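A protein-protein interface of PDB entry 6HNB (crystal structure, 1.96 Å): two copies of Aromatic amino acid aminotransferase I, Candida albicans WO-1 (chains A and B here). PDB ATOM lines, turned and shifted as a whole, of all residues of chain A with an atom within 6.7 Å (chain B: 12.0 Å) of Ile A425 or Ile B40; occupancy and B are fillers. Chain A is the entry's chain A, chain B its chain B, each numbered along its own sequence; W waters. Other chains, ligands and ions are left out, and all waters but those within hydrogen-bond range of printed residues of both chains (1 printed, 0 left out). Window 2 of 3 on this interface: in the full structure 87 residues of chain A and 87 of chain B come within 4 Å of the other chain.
NZ of Lys A480 lies within hydrogen-bond range of OG1 of Thr B41 (3.2 Å).
The backbone carbonyl oxygen (O) of Gly B39 is in hydrogen-bond range of the side-chain amino group (NZ) of Lys A480 (3.1 Å).
N of Leu A430 sits at hydrogen-bond distance from O of Thr B41 (3.0 Å).
The backbone NH of Leu B43 sits at hydrogen-bond distance from the backbone carbonyl oxygen of Leu A430 (2.7 Å).
The backbone carbonyl oxygen of Gly A428 lies close to the backbone carbonyl oxygen of Gly B39, at 3.4 Å.
The backbone NH of Gly B44 lies within hydrogen-bond range of the backbone carbonyl oxygen of Leu A430, at 3.2 Å.
The backbone NH (N) of Thr B41 is in hydrogen-bond range of the backbone carbonyl oxygen (O) of Gly A428 (2.9 Å).
The backbone carbonyl oxygen (O) of Ala A424 is in hydrogen-bond range of the backbone NH (N) of Cys A429, at 3.0 Å.
The backbone carbonyl oxygen (O) of Gly A428 lies within hydrogen-bond range of the side-chain amino group (NZ) of Lys A480 (2.7 Å).
Among the printed residues, merely in contact across the chains: Ile A425 with Tyr B34 (3.8 Å), Ile A425 with Ile B40 (3.7 Å), Gly A428 with Ile B40 (3.4 Å), Cys A429 with Thr B41 (3.4 Å), Cys A429 with Leu B43 (3.98 Å), Leu A430 with Ile B31 (3.9 Å), Leu A430 with Tyr B34 (3.0 Å), Leu A430 with Ile B40 (3.99 Å) and Leu A430 with Phe B42 (3.4 Å).
Val A420 touches none of the printed residues of chain B.
His A421 touches none of the printed residues of chain B.
Glu A422 touches none of the printed residues of chain B.
Ala A424 touches none of the printed residues of chain B.
Ile A425 touches just these residues of chain B: Tyr B34 (3.8 Å) and Ile B40 (3.7 Å).
Of chain B, only Gly B39, Ile B40 and Thr B41 come within 4 Å of Gly A428.
Of the printed residues of chain B, Lys A480 touches Gly B39 (3.1 Å) and Thr B41 (3.2 Å).
Leu B28 touches none of the printed residues of chain A.
Of the printed residues of chain A, Tyr B34 touches Ile A425 and Leu A430.
Printed residues of chain A within 4 Å of Ile B40: Ile A425, Gly A428 and Leu A430.
Of the printed residues of chain A, Phe B42 touches Leu A430.
The nearest residue of chain B that does not touch Ile A425 is Ile B31 (5.9 Å).
The nearest printed residue of chain A that does not touch Ile B40 is Lys A480 (4.5 Å).
Hydrophobic or aromatic side chains of chain B that line the printed part of chain A: Ile B31, Tyr B34, Ile B40, Phe B42 and Leu B43.
Hydrophobic or aromatic side chains of chain A that line the printed part of chain B: Ile A425 and Leu A430.
Among the printed residues, 16 pairs touch across the chains.
No position is printed for both chains.
Of the 16 pairs that touch across the chains among the printed residues, none has its exchanged pair printed and touching as well.
Water W1 bridges a ring nitrogen (NE2) of His A421 (2.9 Å) and the backbone carbonyl oxygen (O) of Gly B30 (3.2 Å).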
ATOM      1  N   VAL A 420       1.256 -21.510  -5.762  1.00  0.00           N
ATOM      2  CA  VAL A 420       2.553 -20.954  -6.230  1.00  0.00           C
ATOM      3  C   VAL A 420       2.619 -21.080  -7.752  1.00  0.00           C
ATOM      4  O   VAL A 420       3.033 -20.104  -8.407  1.00  0.00           O
ATOM      5  CB  VAL A 420       3.741 -21.624  -5.528  1.00  0.00           C
ATOM      6  CG1 VAL A 420       5.063 -21.246  -6.170  1.00  0.00           C
ATOM      7  CG2 VAL A 420       3.727 -21.288  -4.049  1.00  0.00           C
ATOM      8  N   HIS A 421       2.250 -22.234  -8.297  1.00  0.00           N
ATOM      9  CA  HIS A 421       2.207 -22.455  -9.766  1.00  0.00           C
ATOM     10  C   HIS A 421       1.349 -21.358 -10.430  1.00  0.00           C
ATOM     11  O   HIS A 421       1.815 -20.739 -11.454  1.00  0.00           O
ATOM     12  CB  HIS A 421       1.685 -23.869 -10.043  1.00  0.00           C
ATOM     13  CG  HIS A 421       1.733 -24.280 -11.471  1.00  0.00           C
ATOM     14  ND1 HIS A 421       2.886 -24.181 -12.242  1.00  0.00           N
ATOM     15  CD2 HIS A 421       0.779 -24.828 -12.251  1.00  0.00           C
ATOM     16  CE1 HIS A 421       2.610 -24.646 -13.451  1.00  0.00           C
ATOM     17  NE2 HIS A 421       1.313 -25.037 -13.488  1.00  0.00           N
ATOM     18  N   GLU A 422       0.126 -21.137  -9.921  1.00  0.00           N
ATOM     19  CA  GLU A 422      -0.807 -20.114 -10.498  1.00  0.00           C
ATOM     20  C   GLU A 422      -0.179 -18.717 -10.383  1.00  0.00           C
ATOM     21  O   GLU A 422      -0.239 -17.960 -11.389  1.00  0.00           O
ATOM     22  CB  GLU A 422      -2.193 -20.154  -9.845  1.00  0.00           C
ATOM     23  CG  GLU A 422      -2.993 -21.415 -10.144  1.00  0.00           C
ATOM     24  CD  GLU A 422      -4.171 -21.690  -9.211  1.00  0.00           C
ATOM     25  OE1 GLU A 422      -4.822 -20.702  -8.746  1.00  0.00           O
ATOM     26  OE2 GLU A 422      -4.452 -22.896  -8.942  1.00  0.00           O
ATOM     27  N   GLN A 423       0.380 -18.365  -9.216  1.00  0.00           N
ATOM     28  CA  GLN A 423       1.043 -17.054  -9.035  1.00  0.00           C
ATOM     29  C   GLN A 423       2.233 -16.947 -10.010  1.00  0.00           C
ATOM     30  O   GLN A 423       2.420 -15.873 -10.618  1.00  0.00           O
ATOM     31  CB  GLN A 423       1.465 -16.838  -7.587  1.00  0.00           C
ATOM     32  CG  GLN A 423       2.110 -15.480  -7.358  1.00  0.00           C
ATOM     33  CD  GLN A 423       1.104 -14.350  -7.457  1.00  0.00           C
ATOM     34  OE1 GLN A 423       1.317 -13.360  -8.146  1.00  0.00           O
ATOM     35  NE2 GLN A 423      -0.014 -14.502  -6.772  1.00  0.00           N
ATOM     36  N   ALA A 424       3.018 -18.010 -10.200  1.00  0.00           N
ATOM     37  CA  ALA A 424       4.157 -17.976 -11.145  1.00  0.00           C
ATOM     38  C   ALA A 424       3.619 -17.673 -12.549  1.00  0.00           C
ATOM     39  O   ALA A 424       4.124 -16.716 -13.183  1.00  0.00           O
ATOM     40  CB  ALA A 424       4.945 -19.255 -11.081  1.00  0.00           C
ATOM     41  N   ILE A 425       2.585 -18.391 -12.997  1.00  0.00           N
ATOM     42  CA  ILE A 425       1.957 -18.135 -14.326  1.00  0.00           C
ATOM     43  C   ILE A 425       1.543 -16.642 -14.411  1.00  0.00           C
ATOM     44  O   ILE A 425       1.936 -15.976 -15.378  1.00  0.00           O
ATOM     45  CB  ILE A 425       0.794 -19.106 -14.599  1.00  0.00           C
ATOM     46  CG1 ILE A 425       1.291 -20.548 -14.773  1.00  0.00           C
ATOM     47  CG2 ILE A 425      -0.011 -18.645 -15.811  1.00  0.00           C
ATOM     48  CD1 ILE A 425       0.243 -21.606 -14.512  1.00  0.00           C
ATOM     49  N   LYS A 426       0.848 -16.125 -13.401  1.00  0.00           N
ATOM     50  CA  LYS A 426       0.421 -14.700 -13.312  1.00  0.00           C
ATOM     51  C   LYS A 426       1.620 -13.734 -13.370  1.00  0.00           C
ATOM     52  O   LYS A 426       1.472 -12.646 -13.955  1.00  0.00           O
ATOM     53  CB  LYS A 426      -0.386 -14.502 -12.026  1.00  0.00           C
ATOM     54  CG  LYS A 426      -0.674 -13.050 -11.683  1.00  0.00           C
ATOM     55  CD  LYS A 426      -1.809 -12.892 -10.695  1.00  0.00           C
ATOM     56  CE  LYS A 426      -2.138 -11.440 -10.409  1.00  0.00           C
ATOM     57  NZ  LYS A 426      -2.875 -11.320  -9.135  1.00  0.00           N
ATOM     58  N   GLN A 427       2.780 -14.092 -12.810  1.00  0.00           N
ATOM     59  CA  GLN A 427       3.984 -13.217 -12.868  1.00  0.00           C
ATOM     60  C   GLN A 427       4.718 -13.400 -14.202  1.00  0.00           C
ATOM     61  O   GLN A 427       5.676 -12.675 -14.439  1.00  0.00           O
ATOM     62  CB  GLN A 427       4.914 -13.525 -11.703  1.00  0.00           C
ATOM     63  CG  GLN A 427       4.232 -13.347 -10.358  1.00  0.00           C
ATOM     64  CD  GLN A 427       4.075 -11.901  -9.954  1.00  0.00           C
ATOM     65  OE1 GLN A 427       4.682 -10.999 -10.533  1.00  0.00           O
ATOM     66  NE2 GLN A 427       3.264 -11.682  -8.932  1.00  0.00           N
ATOM     67  N   GLY A 428       4.302 -14.354 -15.029  1.00  0.00           N
ATOM     68  CA  GLY A 428       4.867 -14.583 -16.374  1.00  0.00           C
ATOM     69  C   GLY A 428       6.010 -15.600 -16.385  1.00  0.00           C
ATOM     70  O   GLY A 428       6.920 -15.465 -17.217  1.00  0.00           O
ATOM     71  N   CYS A 429       6.003 -16.589 -15.488  1.00  0.00           N
ATOM     72  CA  CYS A 429       7.059 -17.636 -15.457  1.00  0.00           C
ATOM     73  C   CYS A 429       6.383 -18.975 -15.201  1.00  0.00           C
ATOM     74  O   CYS A 429       5.375 -19.029 -14.504  1.00  0.00           O
ATOM     75  CB  CYS A 429       8.086 -17.361 -14.356  1.00  0.00           C
ATOM     76  SG  CYS A 429       9.484 -18.521 -14.244  1.00  0.00           S
ATOM     77  N   LEU A 430       6.885 -20.016 -15.833  1.00  0.00           N
ATOM     78  CA  LEU A 430       6.254 -21.340 -15.740  1.00  0.00           C
ATOM     79  C   LEU A 430       7.342 -22.371 -15.460  1.00  0.00           C
ATOM     80  O   LEU A 430       8.318 -22.468 -16.244  1.00  0.00           O
ATOM     81  CB  LEU A 430       5.511 -21.570 -17.052  1.00  0.00           C
ATOM     82  CG  LEU A 430       4.650 -22.825 -17.130  1.00  0.00           C
ATOM     83  CD1 LEU A 430       3.658 -22.907 -16.004  1.00  0.00           C
ATOM     84  CD2 LEU A 430       3.903 -22.816 -18.430  1.00  0.00           C
ATOM     85  N   LEU A 431       7.174 -23.074 -14.348  1.00  0.00           N
ATOM     86  CA  LEU A 431       8.007 -24.220 -13.936  1.00  0.00           C
ATOM     87  C   LEU A 431       7.056 -25.404 -13.805  1.00  0.00           C
ATOM     88  O   LEU A 431       5.839 -25.167 -13.865  1.00  0.00           O
ATOM     89  CB  LEU A 431       8.738 -23.879 -12.635  1.00  0.00           C
ATOM     90  CG  LEU A 431      10.050 -23.108 -12.807  1.00  0.00           C
ATOM     91  CD1 LEU A 431       9.812 -21.632 -13.052  1.00  0.00           C
ATOM     92  CD2 LEU A 431      10.946 -23.278 -11.595  1.00  0.00           C
ATOM     93  N   LYS A 480      10.916 -13.321 -11.957  1.00  0.00           N
ATOM     94  CA  LYS A 480       9.436 -13.468 -11.922  1.00  0.00           C
ATOM     95  C   LYS A 480       9.035 -14.551 -10.905  1.00  0.00           C
ATOM     96  O   LYS A 480       8.070 -14.339 -10.135  1.00  0.00           O
ATOM     97  CB  LYS A 480       8.921 -13.680 -13.347  1.00  0.00           C
ATOM     98  CG  LYS A 480       8.897 -12.407 -14.198  1.00  0.00           C
ATOM     99  CD  LYS A 480       9.195 -12.612 -15.688  1.00  0.00           C
ATOM    100  CE  LYS A 480       7.984 -12.618 -16.604  1.00  0.00           C
ATOM    101  NZ  LYS A 480       8.271 -13.229 -17.938  1.00  0.00           N
ATOM    102  N   ALA A 484       6.702 -14.302  -7.492  1.00  0.00           N
ATOM    103  CA  ALA A 484       5.586 -15.245  -7.289  1.00  0.00           C
ATOM    104  C   ALA A 484       5.701 -15.864  -5.891  1.00  0.00           C
ATOM    105  O   ALA A 484       4.711 -15.897  -5.204  1.00  0.00           O
ATOM    106  CB  ALA A 484       5.605 -16.295  -8.373  1.00  0.00           C
ATOM    107  N   PRO B  27       1.323 -35.698 -18.018  1.00  0.00           N
ATOM    108  CA  PRO B  27       0.796 -34.540 -17.278  1.00  0.00           C
ATOM    109  C   PRO B  27       1.436 -33.172 -17.623  1.00  0.00           C
ATOM    110  O   PRO B  27       0.945 -32.172 -17.139  1.00  0.00           O
ATOM    111  CB  PRO B  27       1.080 -34.885 -15.804  1.00  0.00           C
ATOM    112  CG  PRO B  27       2.243 -35.876 -15.867  1.00  0.00           C
ATOM    113  CD  PRO B  27       1.994 -36.673 -17.136  1.00  0.00           C
ATOM    114  N   LEU B  28       2.490 -33.139 -18.451  1.00  0.00           N
ATOM    115  CA  LEU B  28       3.176 -31.899 -18.915  1.00  0.00           C
ATOM    116  C   LEU B  28       2.553 -31.379 -20.217  1.00  0.00           C
ATOM    117  O   LEU B  28       2.983 -30.317 -20.691  1.00  0.00           O
ATOM    118  CB  LEU B  28       4.670 -32.187 -19.097  1.00  0.00           C
ATOM    119  CG  LEU B  28       5.510 -32.068 -17.822  1.00  0.00           C
ATOM    120  CD1 LEU B  28       5.081 -33.091 -16.790  1.00  0.00           C
ATOM    121  CD2 LEU B  28       6.985 -32.230 -18.135  1.00  0.00           C
ATOM    122  N   LYS B  29       1.596 -32.115 -20.788  1.00  0.00           N
ATOM    123  CA  LYS B  29       0.751 -31.664 -21.929  1.00  0.00           C
ATOM    124  C   LYS B  29       0.014 -30.383 -21.511  1.00  0.00           C
ATOM    125  O   LYS B  29       0.031 -29.414 -22.293  1.00  0.00           O
ATOM    126  CB  LYS B  29      -0.209 -32.786 -22.339  1.00  0.00           C
ATOM    127  CG  LYS B  29      -1.392 -32.376 -23.211  1.00  0.00           C
ATOM    128  CD  LYS B  29      -2.629 -33.244 -22.996  1.00  0.00           C
ATOM    129  CE  LYS B  29      -3.924 -32.548 -23.349  1.00  0.00           C
ATOM    130  NZ  LYS B  29      -3.937 -32.124 -24.769  1.00  0.00           N
ATOM    131  N   GLY B  30      -0.574 -30.375 -20.310  1.00  0.00           N
ATOM    132  CA  GLY B  30      -1.300 -29.221 -19.745  1.00  0.00           C
ATOM    133  C   GLY B  30      -0.380 -28.153 -19.156  1.00  0.00           C
ATOM    134  O   GLY B  30      -0.736 -27.602 -18.069  1.00  0.00           O
ATOM    135  N   ILE B  31       0.779 -27.902 -19.786  1.00  0.00           N
ATOM    136  CA  ILE B  31       1.513 -26.600 -19.727  1.00  0.00           C
ATOM    137  C   ILE B  31       2.000 -26.263 -21.134  1.00  0.00           C
ATOM    138  O   ILE B  31       2.663 -25.227 -21.279  1.00  0.00           O
ATOM    139  CB  ILE B  31       2.687 -26.594 -18.717  1.00  0.00           C
ATOM    140  CG1 ILE B  31       3.631 -27.787 -18.894  1.00  0.00           C
ATOM    141  CG2 ILE B  31       2.184 -26.469 -17.282  1.00  0.00           C
ATOM    142  CD1 ILE B  31       4.895 -27.684 -18.063  1.00  0.00           C
ATOM    143  N   PHE B  32       1.695 -27.098 -22.135  1.00  0.00           N
ATOM    144  CA  PHE B  32       2.157 -26.876 -23.529  1.00  0.00           C
ATOM    145  C   PHE B  32       1.548 -25.568 -24.048  1.00  0.00           C
ATOM    146  O   PHE B  32       2.254 -24.846 -24.764  1.00  0.00           O
ATOM    147  CB  PHE B  32       1.822 -28.043 -24.468  1.00  0.00           C
ATOM    148  CG  PHE B  32       2.305 -27.821 -25.883  1.00  0.00           C
ATOM    149  CD1 PHE B  32       3.663 -27.854 -26.183  1.00  0.00           C
ATOM    150  CD2 PHE B  32       1.416 -27.504 -26.904  1.00  0.00           C
ATOM    151  CE1 PHE B  32       4.114 -27.614 -27.475  1.00  0.00           C
ATOM    152  CE2 PHE B  32       1.870 -27.266 -28.193  1.00  0.00           C
ATOM    153  CZ  PHE B  32       3.216 -27.322 -28.478  1.00  0.00           C
ATOM    154  N   LYS B  33       0.298 -25.260 -23.691  1.00  0.00           N
ATOM    155  CA  LYS B  33      -0.368 -24.013 -24.150  1.00  0.00           C
ATOM    156  C   LYS B  33       0.572 -22.834 -23.887  1.00  0.00           C
ATOM    157  O   LYS B  33       0.818 -22.072 -24.844  1.00  0.00           O
ATOM    158  CB  LYS B  33      -1.744 -23.829 -23.509  1.00  0.00           C
ATOM    159  CG  LYS B  33      -1.768 -23.713 -22.001  1.00  0.00           C
ATOM    160  CD  LYS B  33      -3.159 -23.857 -21.440  1.00  0.00           C
ATOM    161  CE  LYS B  33      -3.253 -23.425 -19.996  1.00  0.00           C
ATOM    162  NZ  LYS B  33      -4.507 -23.897 -19.368  1.00  0.00           N
ATOM    163  N   TYR B  34       1.164 -22.756 -22.685  1.00  0.00           N
ATOM    164  CA  TYR B  34       2.016 -21.624 -22.241  1.00  0.00           C
ATOM    165  C   TYR B  34       3.354 -21.615 -22.987  1.00  0.00           C
ATOM    166  O   TYR B  34       4.111 -20.664 -22.774  1.00  0.00           O
ATOM    167  CB  TYR B  34       2.276 -21.695 -20.740  1.00  0.00           C
ATOM    168  CG  TYR B  34       1.043 -21.664 -19.872  1.00  0.00           C
ATOM    169  CD1 TYR B  34       0.227 -20.546 -19.838  1.00  0.00           C
ATOM    170  CD2 TYR B  34       0.711 -22.736 -19.052  1.00  0.00           C
ATOM    171  CE1 TYR B  34      -0.888 -20.493 -19.020  1.00  0.00           C
ATOM    172  CE2 TYR B  34      -0.408 -22.699 -18.232  1.00  0.00           C
ATOM    173  CZ  TYR B  34      -1.210 -21.568 -18.212  1.00  0.00           C
ATOM    174  OH  TYR B  34      -2.326 -21.518 -17.425  1.00  0.00           O
ATOM    175  N   TYR B  35       3.637 -22.607 -23.839  1.00  0.00           N
ATOM    176  CA  TYR B  35       4.906 -22.696 -24.612  1.00  0.00           C
ATOM    177  C   TYR B  35       4.861 -21.687 -25.766  1.00  0.00           C
ATOM    178  O   TYR B  35       3.762 -21.485 -26.339  1.00  0.00           O
ATOM    179  CB  TYR B  35       5.160 -24.118 -25.127  1.00  0.00           C
ATOM    180  CG  TYR B  35       6.490 -24.295 -25.817  1.00  0.00           C
ATOM    181  CD1 TYR B  35       7.675 -24.194 -25.107  1.00  0.00           C
ATOM    182  CD2 TYR B  35       6.569 -24.542 -27.181  1.00  0.00           C
ATOM    183  CE1 TYR B  35       8.906 -24.343 -25.726  1.00  0.00           C
ATOM    184  CE2 TYR B  35       7.792 -24.688 -27.819  1.00  0.00           C
ATOM    185  CZ  TYR B  35       8.965 -24.591 -27.087  1.00  0.00           C
ATOM    186  OH  TYR B  35      10.177 -24.737 -27.701  1.00  0.00           O
ATOM    187  N   LYS B  36       6.015 -21.079 -26.082  1.00  0.00           N
ATOM    188  CA  LYS B  36       6.174 -20.074 -27.170  1.00  0.00           C
ATOM    189  C   LYS B  36       4.914 -19.202 -27.213  1.00  0.00           C
ATOM    190  O   LYS B  36       4.231 -19.220 -28.250  1.00  0.00           O
ATOM    191  CB  LYS B  36       6.416 -20.762 -28.520  1.00  0.00           C
ATOM    192  N   GLN B  37       4.590 -18.531 -26.100  1.00  0.00           N
ATOM    193  CA  GLN B  37       3.502 -17.519 -26.007  1.00  0.00           C
ATOM    194  C   GLN B  37       4.052 -16.335 -25.209  1.00  0.00           C
ATOM    195  O   GLN B  37       4.401 -16.468 -24.038  1.00  0.00           O
ATOM    196  CB  GLN B  37       2.210 -18.154 -25.470  1.00  0.00           C
ATOM    197  CG  GLN B  37       1.982 -18.005 -23.969  1.00  0.00           C
ATOM    198  CD  GLN B  37       0.639 -17.412 -23.624  1.00  0.00           C
ATOM    199  OE1 GLN B  37       0.024 -16.719 -24.433  1.00  0.00           O
ATOM    200  NE2 GLN B  37       0.184 -17.666 -22.404  1.00  0.00           N
ATOM    201  N   PRO B  38       4.215 -15.143 -25.831  1.00  0.00           N
ATOM    202  CA  PRO B  38       4.916 -14.032 -25.182  1.00  0.00           C
ATOM    203  C   PRO B  38       4.218 -13.557 -23.893  1.00  0.00           C
ATOM    204  O   PRO B  38       3.005 -13.731 -23.723  1.00  0.00           O
ATOM    205  CB  PRO B  38       4.984 -12.945 -26.268  1.00  0.00           C
ATOM    206  CG  PRO B  38       3.859 -13.292 -27.227  1.00  0.00           C
ATOM    207  CD  PRO B  38       3.743 -14.802 -27.180  1.00  0.00           C
ATOM    208  N   GLY B  39       5.021 -12.983 -23.000  1.00  0.00           N
ATOM    209  CA  GLY B  39       4.656 -12.708 -21.598  1.00  0.00           C
ATOM    210  C   GLY B  39       5.239 -13.769 -20.678  1.00  0.00           C
ATOM    211  O   GLY B  39       5.626 -13.405 -19.547  1.00  0.00           O
ATOM    212  N   ILE B  40       5.323 -15.025 -21.151  1.00  0.00           N
ATOM    213  CA  ILE B  40       5.690 -16.210 -20.315  1.00  0.00           C
ATOM    214  C   ILE B  40       7.128 -16.609 -20.617  1.00  0.00           C
ATOM    215  O   ILE B  40       7.438 -16.871 -21.790  1.00  0.00           O
ATOM    216  CB  ILE B  40       4.727 -17.394 -20.534  1.00  0.00           C
ATOM    217  CG1 ILE B  40       3.272 -16.982 -20.309  1.00  0.00           C
ATOM    218  CG2 ILE B  40       5.099 -18.586 -19.662  1.00  0.00           C
ATOM    219  CD1 ILE B  40       2.992 -16.454 -18.935  1.00  0.00           C
ATOM    220  N   THR B  41       7.980 -16.624 -19.596  1.00  0.00           N
ATOM    221  CA  THR B  41       9.253 -17.366 -19.653  1.00  0.00           C
ATOM    222  C   THR B  41       8.926 -18.807 -19.264  1.00  0.00           C
ATOM    223  O   THR B  41       8.630 -19.047 -18.070  1.00  0.00           O
ATOM    224  CB  THR B  41      10.333 -16.747 -18.772  1.00  0.00           C
ATOM    225  OG1 THR B  41      10.368 -15.346 -19.040  1.00  0.00           O
ATOM    226  CG2 THR B  41      11.685 -17.378 -19.036  1.00  0.00           C
ATOM    227  N   PHE B  42       8.931 -19.691 -20.253  1.00  0.00           N
ATOM    228  CA  PHE B  42       8.570 -21.126 -20.157  1.00  0.00           C
ATOM    229  C   PHE B  42       9.797 -21.934 -19.745  1.00  0.00           C
ATOM    230  O   PHE B  42      10.631 -22.191 -20.615  1.00  0.00           O
ATOM    231  CB  PHE B  42       8.054 -21.637 -21.507  1.00  0.00           C
ATOM    232  CG  PHE B  42       7.527 -23.040 -21.418  1.00  0.00           C
ATOM    233  CD1 PHE B  42       6.276 -23.271 -20.881  1.00  0.00           C
ATOM    234  CD2 PHE B  42       8.297 -24.128 -21.798  1.00  0.00           C
ATOM    235  CE1 PHE B  42       5.791 -24.563 -20.752  1.00  0.00           C
ATOM    236  CE2 PHE B  42       7.798 -25.414 -21.691  1.00  0.00           C
ATOM    237  CZ  PHE B  42       6.552 -25.629 -21.158  1.00  0.00           C
ATOM    238  N   LEU B  43       9.906 -22.311 -18.467  1.00  0.00           N
ATOM    239  CA  LEU B  43      11.036 -23.120 -17.941  1.00  0.00           C
ATOM    240  C   LEU B  43      10.570 -24.537 -17.569  1.00  0.00           C
ATOM    241  O   LEU B  43      11.326 -25.253 -16.863  1.00  0.00           O
ATOM    242  CB  LEU B  43      11.634 -22.404 -16.723  1.00  0.00           C
ATOM    243  CG  LEU B  43      12.088 -20.963 -16.971  1.00  0.00           C
ATOM    244  CD1 LEU B  43      12.699 -20.345 -15.707  1.00  0.00           C
ATOM    245  CD2 LEU B  43      13.057 -20.902 -18.147  1.00  0.00           C
ATOM    246  N   GLY B  44       9.389 -24.948 -18.030  1.00  0.00           N
ATOM    247  CA  GLY B  44       8.722 -26.159 -17.513  1.00  0.00           C
ATOM    248  C   GLY B  44       8.966 -27.378 -18.379  1.00  0.00           C
ATOM    249  O   GLY B  44       8.446 -28.450 -18.025  1.00  0.00           O
ATOM    250  N   GLY B  45       9.719 -27.219 -19.472  1.00  0.00           N
ATOM    251  CA  GLY B  45       9.945 -28.271 -20.484  1.00  0.00           C
ATOM    252  C   GLY B  45      11.273 -28.987 -20.324  1.00  0.00           C
ATOM    253  O   GLY B  45      11.969 -28.754 -19.287  1.00  0.00           O
HETATM  254  O   HOH W   1      -0.755 -25.737 -15.408  1.00  0.00           O
